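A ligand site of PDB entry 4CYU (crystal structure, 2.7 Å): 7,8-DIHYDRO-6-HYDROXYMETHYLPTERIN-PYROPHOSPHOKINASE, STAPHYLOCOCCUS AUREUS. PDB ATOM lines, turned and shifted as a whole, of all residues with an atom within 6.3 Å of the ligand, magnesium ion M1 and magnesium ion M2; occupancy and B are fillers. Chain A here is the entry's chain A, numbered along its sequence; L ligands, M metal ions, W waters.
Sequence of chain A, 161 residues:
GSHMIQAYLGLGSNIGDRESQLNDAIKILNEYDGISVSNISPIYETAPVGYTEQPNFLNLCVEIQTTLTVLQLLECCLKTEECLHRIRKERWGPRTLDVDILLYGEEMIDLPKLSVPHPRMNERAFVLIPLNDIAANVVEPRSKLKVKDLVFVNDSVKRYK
Magnesium ion M2 is bound by the side-chain carboxylate of Asp 98 (2.1 Å), an oxygen (O1) of the ligand (2.1 Å), the side-chain carboxylate of Asp 100 (2.4 Å) and an oxygen (O4) of the ligand (2.4 Å).
The nearest printed residue that does not touch magnesium ion M1 is Val 99 (4.2 Å).
Merely in contact with the ligand: Leu 74, Glu 81, Val 99 and Leu 114. Hydrophobic or aromatic side chains that line the ligand: Leu 74, Ile 101, Leu 114 and His 118.
The guanidinium group (NH2) of Arg 95 lies within salt-bridge range of an oxygen (O5) of the ligand, at 2.4 Å. O of Lys 113 sits at hydrogen-bond distance from O12 of the ligand (2.7 Å). NH2 of Arg 124 is in salt-bridge range of O2 of the ligand. The backbone NH (N) of Ile 101 lies within hydrogen-bond range of a nitrogen (N4) of the ligand, 2.9 Å away. The backbone carbonyl oxygen (O) of Ile 101 lies within hydrogen-bond range of a nitrogen (N3) of the ligand, at 2.7 Å. The backbone NH of Ser 115 lies within hydrogen-bond range of a nitrogen (N2) of the ligand. A nitrogen (N3) of the ligand is in hydrogen-bond range of the backbone carbonyl oxygen of Ser 115, 2.9 Å away. An oxygen (O3) of the ligand is in hydrogen-bond range of a ring nitrogen (NE2) of His 118. An oxygen (O2) of the ligand lies within salt-bridge range of the guanidinium group of Arg 120 (2.9 Å).
Two residues have an atom within 4 Å of magnesium ion M2: Asp 98 and Asp 100. The nearest printed residue that does not touch magnesium ion M2 is Arg 124 (4.02 Å).
The side-chain carboxylate of Asp 98 sits close to the guanidinium group of Arg 95, at 3.3 Å. NH1 of Arg 95 is in salt-bridge range of OE1 of Glu 81, at 3.0 Å. A ring nitrogen (ND1) of His 118 lies close to the backbone NH (N) of Arg 120. N of His 118 lies within hydrogen-bond range of O of Leu 102 (3.1 Å). OE2 of Glu 81 is in hydrogen-bond range of N of Val 99.
Magnesium ion M1 is bound by O7 of the ligand (2.0 Å), OD1 of Asp 100 (2.0 Å), O4 of the ligand (2.2 Å), water W1 (2.3 Å) and OD1 of Asp 98 (2.4 Å).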
ATOM      1  N   LEU A  74      21.695 -20.254  -1.675  1.00  0.00           N
ATOM      2  CA  LEU A  74      23.025 -20.630  -1.190  1.00  0.00           C
ATOM      3  C   LEU A  74      24.086 -20.573  -2.296  1.00  0.00           C
ATOM      4  O   LEU A  74      25.180 -20.057  -2.073  1.00  0.00           O
ATOM      5  CB  LEU A  74      23.007 -22.020  -0.588  1.00  0.00           C
ATOM      6  CG  LEU A  74      24.357 -22.507  -0.032  1.00  0.00           C
ATOM      7  CD1 LEU A  74      24.857 -21.603   1.078  1.00  0.00           C
ATOM      8  CD2 LEU A  74      24.246 -23.941   0.453  1.00  0.00           C
ATOM      9  N   CYS A  77      25.038 -17.029  -2.963  1.00  0.00           N
ATOM     10  CA  CYS A  77      25.870 -16.508  -1.876  1.00  0.00           C
ATOM     11  C   CYS A  77      27.315 -16.950  -2.027  1.00  0.00           C
ATOM     12  O   CYS A  77      28.233 -16.138  -1.905  1.00  0.00           O
ATOM     13  CB  CYS A  77      25.335 -16.943  -0.517  1.00  0.00           C
ATOM     14  SG  CYS A  77      23.748 -16.175  -0.091  1.00  0.00           S
ATOM     15  N   LEU A  78      27.515 -18.218  -2.325  1.00  0.00           N
ATOM     16  CA  LEU A  78      28.852 -18.768  -2.491  1.00  0.00           C
ATOM     17  C   LEU A  78      29.556 -18.273  -3.746  1.00  0.00           C
ATOM     18  O   LEU A  78      30.764 -18.103  -3.741  1.00  0.00           O
ATOM     19  CB  LEU A  78      28.836 -20.292  -2.480  1.00  0.00           C
ATOM     20  CG  LEU A  78      28.275 -20.875  -1.193  1.00  0.00           C
ATOM     21  CD1 LEU A  78      28.294 -22.391  -1.283  1.00  0.00           C
ATOM     22  CD2 LEU A  78      29.028 -20.402   0.053  1.00  0.00           C
ATOM     23  N   GLU A  81      30.805 -14.868  -2.782  1.00  0.00           N
ATOM     24  CA  GLU A  81      32.081 -15.023  -2.030  1.00  0.00           C
ATOM     25  C   GLU A  81      33.216 -15.324  -3.009  1.00  0.00           C
ATOM     26  O   GLU A  81      34.267 -14.689  -2.983  1.00  0.00           O
ATOM     27  CB  GLU A  81      32.009 -16.155  -0.983  1.00  0.00           C
ATOM     28  CG  GLU A  81      31.117 -15.894   0.240  1.00  0.00           C
ATOM     29  CD  GLU A  81      31.172 -17.001   1.288  1.00  0.00           C
ATOM     30  OE1 GLU A  81      31.973 -17.952   1.139  1.00  0.00           O
ATOM     31  OE2 GLU A  81      30.423 -16.937   2.281  1.00  0.00           O
ATOM     32  N   ARG A  95      40.153 -15.142   3.383  1.00  0.00           N
ATOM     33  CA  ARG A  95      39.051 -14.793   2.488  1.00  0.00           C
ATOM     34  C   ARG A  95      38.463 -13.435   2.803  1.00  0.00           C
ATOM     35  O   ARG A  95      38.497 -12.932   3.947  1.00  0.00           O
ATOM     36  CB  ARG A  95      37.995 -15.884   2.302  1.00  0.00           C
ATOM     37  CG  ARG A  95      37.302 -16.351   3.546  1.00  0.00           C
ATOM     38  CD  ARG A  95      35.798 -16.427   3.374  1.00  0.00           C
ATOM     39  NE  ARG A  95      35.285 -16.875   4.650  1.00  0.00           N
ATOM     40  CZ  ARG A  95      34.163 -17.528   4.855  1.00  0.00           C
ATOM     41  NH1 ARG A  95      33.344 -17.841   3.849  1.00  0.00           N
ATOM     42  NH2 ARG A  95      33.845 -17.881   6.091  1.00  0.00           N
ATOM     43  N   ASP A  98      32.386 -13.135   3.920  1.00  0.00           N
ATOM     44  CA  ASP A  98      31.500 -14.234   4.315  1.00  0.00           C
ATOM     45  C   ASP A  98      30.077 -13.780   4.090  1.00  0.00           C
ATOM     46  O   ASP A  98      29.662 -12.713   4.543  1.00  0.00           O
ATOM     47  CB  ASP A  98      31.720 -14.626   5.784  1.00  0.00           C
ATOM     48  CG  ASP A  98      30.894 -15.861   6.198  1.00  0.00           C
ATOM     49  OD1 ASP A  98      30.640 -16.778   5.362  1.00  0.00           O
ATOM     50  OD2 ASP A  98      30.518 -15.924   7.391  1.00  0.00           O
ATOM     51  N   VAL A  99      29.324 -14.613   3.370  1.00  0.00           N
ATOM     52  CA  VAL A  99      27.896 -14.407   3.176  1.00  0.00           C
ATOM     53  C   VAL A  99      27.173 -15.597   3.764  1.00  0.00           C
ATOM     54  O   VAL A  99      27.258 -16.701   3.254  1.00  0.00           O
ATOM     55  CB  VAL A  99      27.525 -14.288   1.705  1.00  0.00           C
ATOM     56  CG1 VAL A  99      26.040 -13.972   1.547  1.00  0.00           C
ATOM     57  CG2 VAL A  99      28.365 -13.196   1.051  1.00  0.00           C
ATOM     58  N   ASP A 100      26.460 -15.346   4.849  1.00  0.00           N
ATOM     59  CA  ASP A 100      25.746 -16.387   5.549  1.00  0.00           C
ATOM     60  C   ASP A 100      24.229 -16.160   5.416  1.00  0.00           C
ATOM     61  O   ASP A 100      23.745 -15.034   5.469  1.00  0.00           O
ATOM     62  CB  ASP A 100      26.190 -16.434   7.020  1.00  0.00           C
ATOM     63  CG  ASP A 100      27.592 -16.974   7.197  1.00  0.00           C
ATOM     64  OD1 ASP A 100      28.162 -17.501   6.215  1.00  0.00           O
ATOM     65  OD2 ASP A 100      28.146 -16.906   8.322  1.00  0.00           O
ATOM     66  N   ILE A 101      23.489 -17.242   5.227  1.00  0.00           N
ATOM     67  CA  ILE A 101      22.038 -17.161   5.224  1.00  0.00           C
ATOM     68  C   ILE A 101      21.540 -17.269   6.650  1.00  0.00           C
ATOM     69  O   ILE A 101      21.771 -18.266   7.326  1.00  0.00           O
ATOM     70  CB  ILE A 101      21.382 -18.266   4.393  1.00  0.00           C
ATOM     71  CG1 ILE A 101      21.895 -18.204   2.958  1.00  0.00           C
ATOM     72  CG2 ILE A 101      19.881 -18.074   4.383  1.00  0.00           C
ATOM     73  CD1 ILE A 101      21.332 -19.269   2.036  1.00  0.00           C
ATOM     74  N   LEU A 102      20.829 -16.251   7.091  1.00  0.00           N
ATOM     75  CA  LEU A 102      20.381 -16.185   8.468  1.00  0.00           C
ATOM     76  C   LEU A 102      18.976 -16.721   8.643  1.00  0.00           C
ATOM     77  O   LEU A 102      18.696 -17.533   9.544  1.00  0.00           O
ATOM     78  CB  LEU A 102      20.416 -14.739   8.936  1.00  0.00           C
ATOM     79  CG  LEU A 102      21.790 -14.090   8.870  1.00  0.00           C
ATOM     80  CD1 LEU A 102      21.708 -12.629   9.257  1.00  0.00           C
ATOM     81  CD2 LEU A 102      22.760 -14.819   9.787  1.00  0.00           C
ATOM     82  N   LEU A 111      20.136 -29.587   6.448  1.00  0.00           N
ATOM     83  CA  LEU A 111      20.913 -30.369   5.518  1.00  0.00           C
ATOM     84  C   LEU A 111      22.356 -30.327   5.994  1.00  0.00           C
ATOM     85  O   LEU A 111      22.774 -29.386   6.669  1.00  0.00           O
ATOM     86  CB  LEU A 111      20.800 -29.780   4.117  1.00  0.00           C
ATOM     87  CG  LEU A 111      19.385 -29.783   3.522  1.00  0.00           C
ATOM     88  CD1 LEU A 111      19.269 -28.834   2.348  1.00  0.00           C
ATOM     89  CD2 LEU A 111      19.028 -31.203   3.091  1.00  0.00           C
ATOM     90  N   PRO A 112      23.140 -31.353   5.662  1.00  0.00           N
ATOM     91  CA  PRO A 112      24.583 -31.279   5.923  1.00  0.00           C
ATOM     92  C   PRO A 112      25.220 -30.003   5.373  1.00  0.00           C
ATOM     93  O   PRO A 112      26.067 -29.414   6.027  1.00  0.00           O
ATOM     94  CB  PRO A 112      25.112 -32.522   5.212  1.00  0.00           C
ATOM     95  CG  PRO A 112      23.991 -33.504   5.289  1.00  0.00           C
ATOM     96  CD  PRO A 112      22.731 -32.695   5.186  1.00  0.00           C
ATOM     97  N   LYS A 113      24.821 -29.582   4.181  1.00  0.00           N
ATOM     98  CA  LYS A 113      25.432 -28.402   3.536  1.00  0.00           C
ATOM     99  C   LYS A 113      24.789 -27.074   3.912  1.00  0.00           C
ATOM    100  O   LYS A 113      25.271 -26.023   3.497  1.00  0.00           O
ATOM    101  CB  LYS A 113      25.391 -28.531   1.994  1.00  0.00           C
ATOM    102  CG  LYS A 113      25.891 -29.884   1.472  1.00  0.00           C
ATOM    103  CD  LYS A 113      27.325 -30.166   1.869  1.00  0.00           C
ATOM    104  CE  LYS A 113      28.001 -31.192   0.990  1.00  0.00           C
ATOM    105  NZ  LYS A 113      28.746 -30.509  -0.103  1.00  0.00           N
ATOM    106  N   LEU A 114      23.690 -27.122   4.647  1.00  0.00           N
ATOM    107  CA  LEU A 114      22.881 -25.939   4.890  1.00  0.00           C
ATOM    108  C   LEU A 114      22.021 -26.020   6.160  1.00  0.00           C
ATOM    109  O   LEU A 114      21.194 -26.908   6.302  1.00  0.00           O
ATOM    110  CB  LEU A 114      21.958 -25.673   3.689  1.00  0.00           C
ATOM    111  CG  LEU A 114      21.131 -24.396   3.793  1.00  0.00           C
ATOM    112  CD1 LEU A 114      22.022 -23.186   3.985  1.00  0.00           C
ATOM    113  CD2 LEU A 114      20.254 -24.224   2.566  1.00  0.00           C
ATOM    114  N   SER A 115      22.202 -25.049   7.041  1.00  0.00           N
ATOM    115  CA  SER A 115      21.387 -24.940   8.259  1.00  0.00           C
ATOM    116  C   SER A 115      20.762 -23.590   8.320  1.00  0.00           C
ATOM    117  O   SER A 115      21.452 -22.594   8.426  1.00  0.00           O
ATOM    118  CB  SER A 115      22.251 -25.104   9.520  1.00  0.00           C
ATOM    119  OG  SER A 115      22.665 -26.445   9.692  1.00  0.00           O
ATOM    120  N   VAL A 116      19.441 -23.547   8.280  1.00  0.00           N
ATOM    121  CA  VAL A 116      18.709 -22.291   8.410  1.00  0.00           C
ATOM    122  C   VAL A 116      17.603 -22.504   9.405  1.00  0.00           C
ATOM    123  O   VAL A 116      16.871 -23.469   9.288  1.00  0.00           O
ATOM    124  CB  VAL A 116      18.077 -21.871   7.087  1.00  0.00           C
ATOM    125  CG1 VAL A 116      17.333 -20.570   7.242  1.00  0.00           C
ATOM    126  CG2 VAL A 116      19.143 -21.703   6.029  1.00  0.00           C
ATOM    127  N   PRO A 117      17.440 -21.594  10.376  1.00  0.00           N
ATOM    128  CA  PRO A 117      18.220 -20.403  10.636  1.00  0.00           C
ATOM    129  C   PRO A 117      19.634 -20.713  10.987  1.00  0.00           C
ATOM    130  O   PRO A 117      19.926 -21.787  11.482  1.00  0.00           O
ATOM    131  CB  PRO A 117      17.533 -19.785  11.860  1.00  0.00           C
ATOM    132  CG  PRO A 117      16.145 -20.290  11.780  1.00  0.00           C
ATOM    133  CD  PRO A 117      16.305 -21.693  11.296  1.00  0.00           C
ATOM    134  N   HIS A 118      20.517 -19.762  10.723  1.00  0.00           N
ATOM    135  CA  HIS A 118      21.915 -19.998  10.997  1.00  0.00           C
ATOM    136  C   HIS A 118      21.992 -20.376  12.465  1.00  0.00           C
ATOM    137  O   HIS A 118      21.483 -19.655  13.311  1.00  0.00           O
ATOM    138  CB  HIS A 118      22.754 -18.756  10.735  1.00  0.00           C
ATOM    139  CG  HIS A 118      24.220 -19.042  10.746  1.00  0.00           C
ATOM    140  ND1 HIS A 118      24.933 -19.227  11.910  1.00  0.00           N
ATOM    141  CD2 HIS A 118      25.107 -19.175   9.736  1.00  0.00           C
ATOM    142  CE1 HIS A 118      26.201 -19.456  11.612  1.00  0.00           C
ATOM    143  NE2 HIS A 118      26.339 -19.437  10.300  1.00  0.00           N
ATOM    144  N   PRO A 119      22.613 -21.521  12.756  1.00  0.00           N
ATOM    145  CA  PRO A 119      22.559 -22.073  14.100  1.00  0.00           C
ATOM    146  C   PRO A 119      23.406 -21.357  15.154  1.00  0.00           C
ATOM    147  O   PRO A 119      23.396 -21.785  16.285  1.00  0.00           O
ATOM    148  CB  PRO A 119      23.052 -23.516  13.906  1.00  0.00           C
ATOM    149  CG  PRO A 119      23.871 -23.473  12.681  1.00  0.00           C
ATOM    150  CD  PRO A 119      23.230 -22.458  11.804  1.00  0.00           C
ATOM    151  N   ARG A 120      24.115 -20.305  14.783  1.00  0.00           N
ATOM    152  CA  ARG A 120      24.890 -19.531  15.752  1.00  0.00           C
ATOM    153  C   ARG A 120      24.499 -18.063  15.828  1.00  0.00           C
ATOM    154  O   ARG A 120      25.113 -17.298  16.573  1.00  0.00           O
ATOM    155  CB  ARG A 120      26.391 -19.670  15.454  1.00  0.00           C
ATOM    156  CG  ARG A 120      26.982 -20.978  15.957  1.00  0.00           C
ATOM    157  CD  ARG A 120      28.412 -21.225  15.482  1.00  0.00           C
ATOM    158  NE  ARG A 120      28.504 -21.411  14.037  1.00  0.00           N
ATOM    159  CZ  ARG A 120      28.104 -22.500  13.370  1.00  0.00           C
ATOM    160  NH1 ARG A 120      27.562 -23.542  14.006  1.00  0.00           N
ATOM    161  NH2 ARG A 120      28.219 -22.548  12.049  1.00  0.00           N
ATOM    162  N   ARG A 124      25.469 -14.330  18.641  1.00  0.00           N
ATOM    163  CA  ARG A 124      26.391 -13.371  18.009  1.00  0.00           C
ATOM    164  C   ARG A 124      25.796 -11.976  17.873  1.00  0.00           C
ATOM    165  O   ARG A 124      24.895 -11.746  17.067  1.00  0.00           O
ATOM    166  CB  ARG A 124      26.789 -13.831  16.612  1.00  0.00           C
ATOM    167  CG  ARG A 124      27.670 -15.066  16.561  1.00  0.00           C
ATOM    168  CD  ARG A 124      27.818 -15.567  15.127  1.00  0.00           C
ATOM    169  NE  ARG A 124      28.892 -16.553  14.996  1.00  0.00           N
ATOM    170  CZ  ARG A 124      29.143 -17.290  13.916  1.00  0.00           C
ATOM    171  NH1 ARG A 124      28.389 -17.191  12.827  1.00  0.00           N
ATOM    172  NH2 ARG A 124      30.159 -18.144  13.913  1.00  0.00           N
ATOM    173  N   PHE A 126      27.188  -9.336  16.654  1.00  0.00           N
ATOM    174  CA  PHE A 126      27.537  -8.733  15.377  1.00  0.00           C
ATOM    175  C   PHE A 126      26.583  -9.162  14.259  1.00  0.00           C
ATOM    176  O   PHE A 126      26.658  -8.660  13.124  1.00  0.00           O
ATOM    177  CB  PHE A 126      28.997  -8.974  15.015  1.00  0.00           C
ATOM    178  CG  PHE A 126      29.367 -10.410  14.776  1.00  0.00           C
ATOM    179  CD1 PHE A 126      29.050 -11.039  13.573  1.00  0.00           C
ATOM    180  CD2 PHE A 126      30.095 -11.108  15.727  1.00  0.00           C
ATOM    181  CE1 PHE A 126      29.409 -12.358  13.343  1.00  0.00           C
ATOM    182  CE2 PHE A 126      30.472 -12.432  15.505  1.00  0.00           C
ATOM    183  CZ  PHE A 126      30.123 -13.054  14.303  1.00  0.00           C
HETATM  184  P1  LIG L   1      29.840 -19.647  10.520  1.00  0.00           P
HETATM  185  O1  LIG L   1      29.522 -18.186  10.319  1.00  0.00           O
HETATM  186  O2  LIG L   1      30.057 -20.001  11.964  1.00  0.00           O
HETATM  187  O3  LIG L   1      28.959 -20.642   9.776  1.00  0.00           O
HETATM  188  P2  LIG L   1      31.501 -19.536   8.317  1.00  0.00           P
HETATM  189  O4  LIG L   1      30.547 -18.478   7.875  1.00  0.00           O
HETATM  190  O5  LIG L   1      33.023 -19.088   8.055  1.00  0.00           O
HETATM  191  O6  LIG L   1      31.298 -19.793   9.880  1.00  0.00           O
HETATM  192  P3  LIG L   1      31.835 -20.796   5.681  1.00  0.00           P
HETATM  193  O7  LIG L   1      31.314 -19.510   5.186  1.00  0.00           O
HETATM  194  O8  LIG L   1      33.440 -20.730   5.642  1.00  0.00           O
HETATM  195  C1  LIG L   1      31.292 -21.070   7.405  1.00  0.00           C
HETATM  196  O9  LIG L   1      31.283 -21.944   4.688  1.00  0.00           O
HETATM  197  C2  LIG L   1      30.848 -23.127   5.286  1.00  0.00           C
HETATM  198  C3  LIG L   1      29.857 -23.975   4.517  1.00  0.00           C
HETATM  199  O10 LIG L   1      28.791 -24.069   5.459  1.00  0.00           O
HETATM  200  C4  LIG L   1      29.244 -23.419   3.247  1.00  0.00           C
HETATM  201  O11 LIG L   1      29.901 -23.906   2.086  1.00  0.00           O
HETATM  202  C5  LIG L   1      27.788 -23.851   3.337  1.00  0.00           C
HETATM  203  O12 LIG L   1      27.473 -24.949   2.469  1.00  0.00           O
HETATM  204  C6  LIG L   1      27.571 -24.257   4.802  1.00  0.00           C
HETATM  205  N1  LIG L   1      26.440 -23.550   5.480  1.00  0.00           N
HETATM  206  C7  LIG L   1      25.638 -24.156   6.385  1.00  0.00           C
HETATM  207  N2  LIG L   1      24.663 -23.310   6.829  1.00  0.00           N
HETATM  208  C8  LIG L   1      24.817 -22.153   6.172  1.00  0.00           C
HETATM  209  C9  LIG L   1      24.127 -20.842   6.158  1.00  0.00           C
HETATM  210  N3  LIG L   1      23.051 -20.640   6.947  1.00  0.00           N
HETATM  211  N4  LIG L   1      24.602 -19.866   5.332  1.00  0.00           N
HETATM  212  C10 LIG L   1      25.670 -20.089   4.547  1.00  0.00           C
HETATM  213  N5  LIG L   1      26.354 -21.251   4.527  1.00  0.00           N
HETATM  214  C11 LIG L   1      25.990 -22.309   5.285  1.00  0.00           C
HETATM  215 MG    MG M   1      29.592 -18.897   5.994  1.00  0.00          MG
HETATM  216 MG    MG M   2      30.268 -16.536   9.336  1.00  0.00          MG
HETATM  217  O   HOH W   1      29.253 -18.214   3.802  1.00  0.00           O
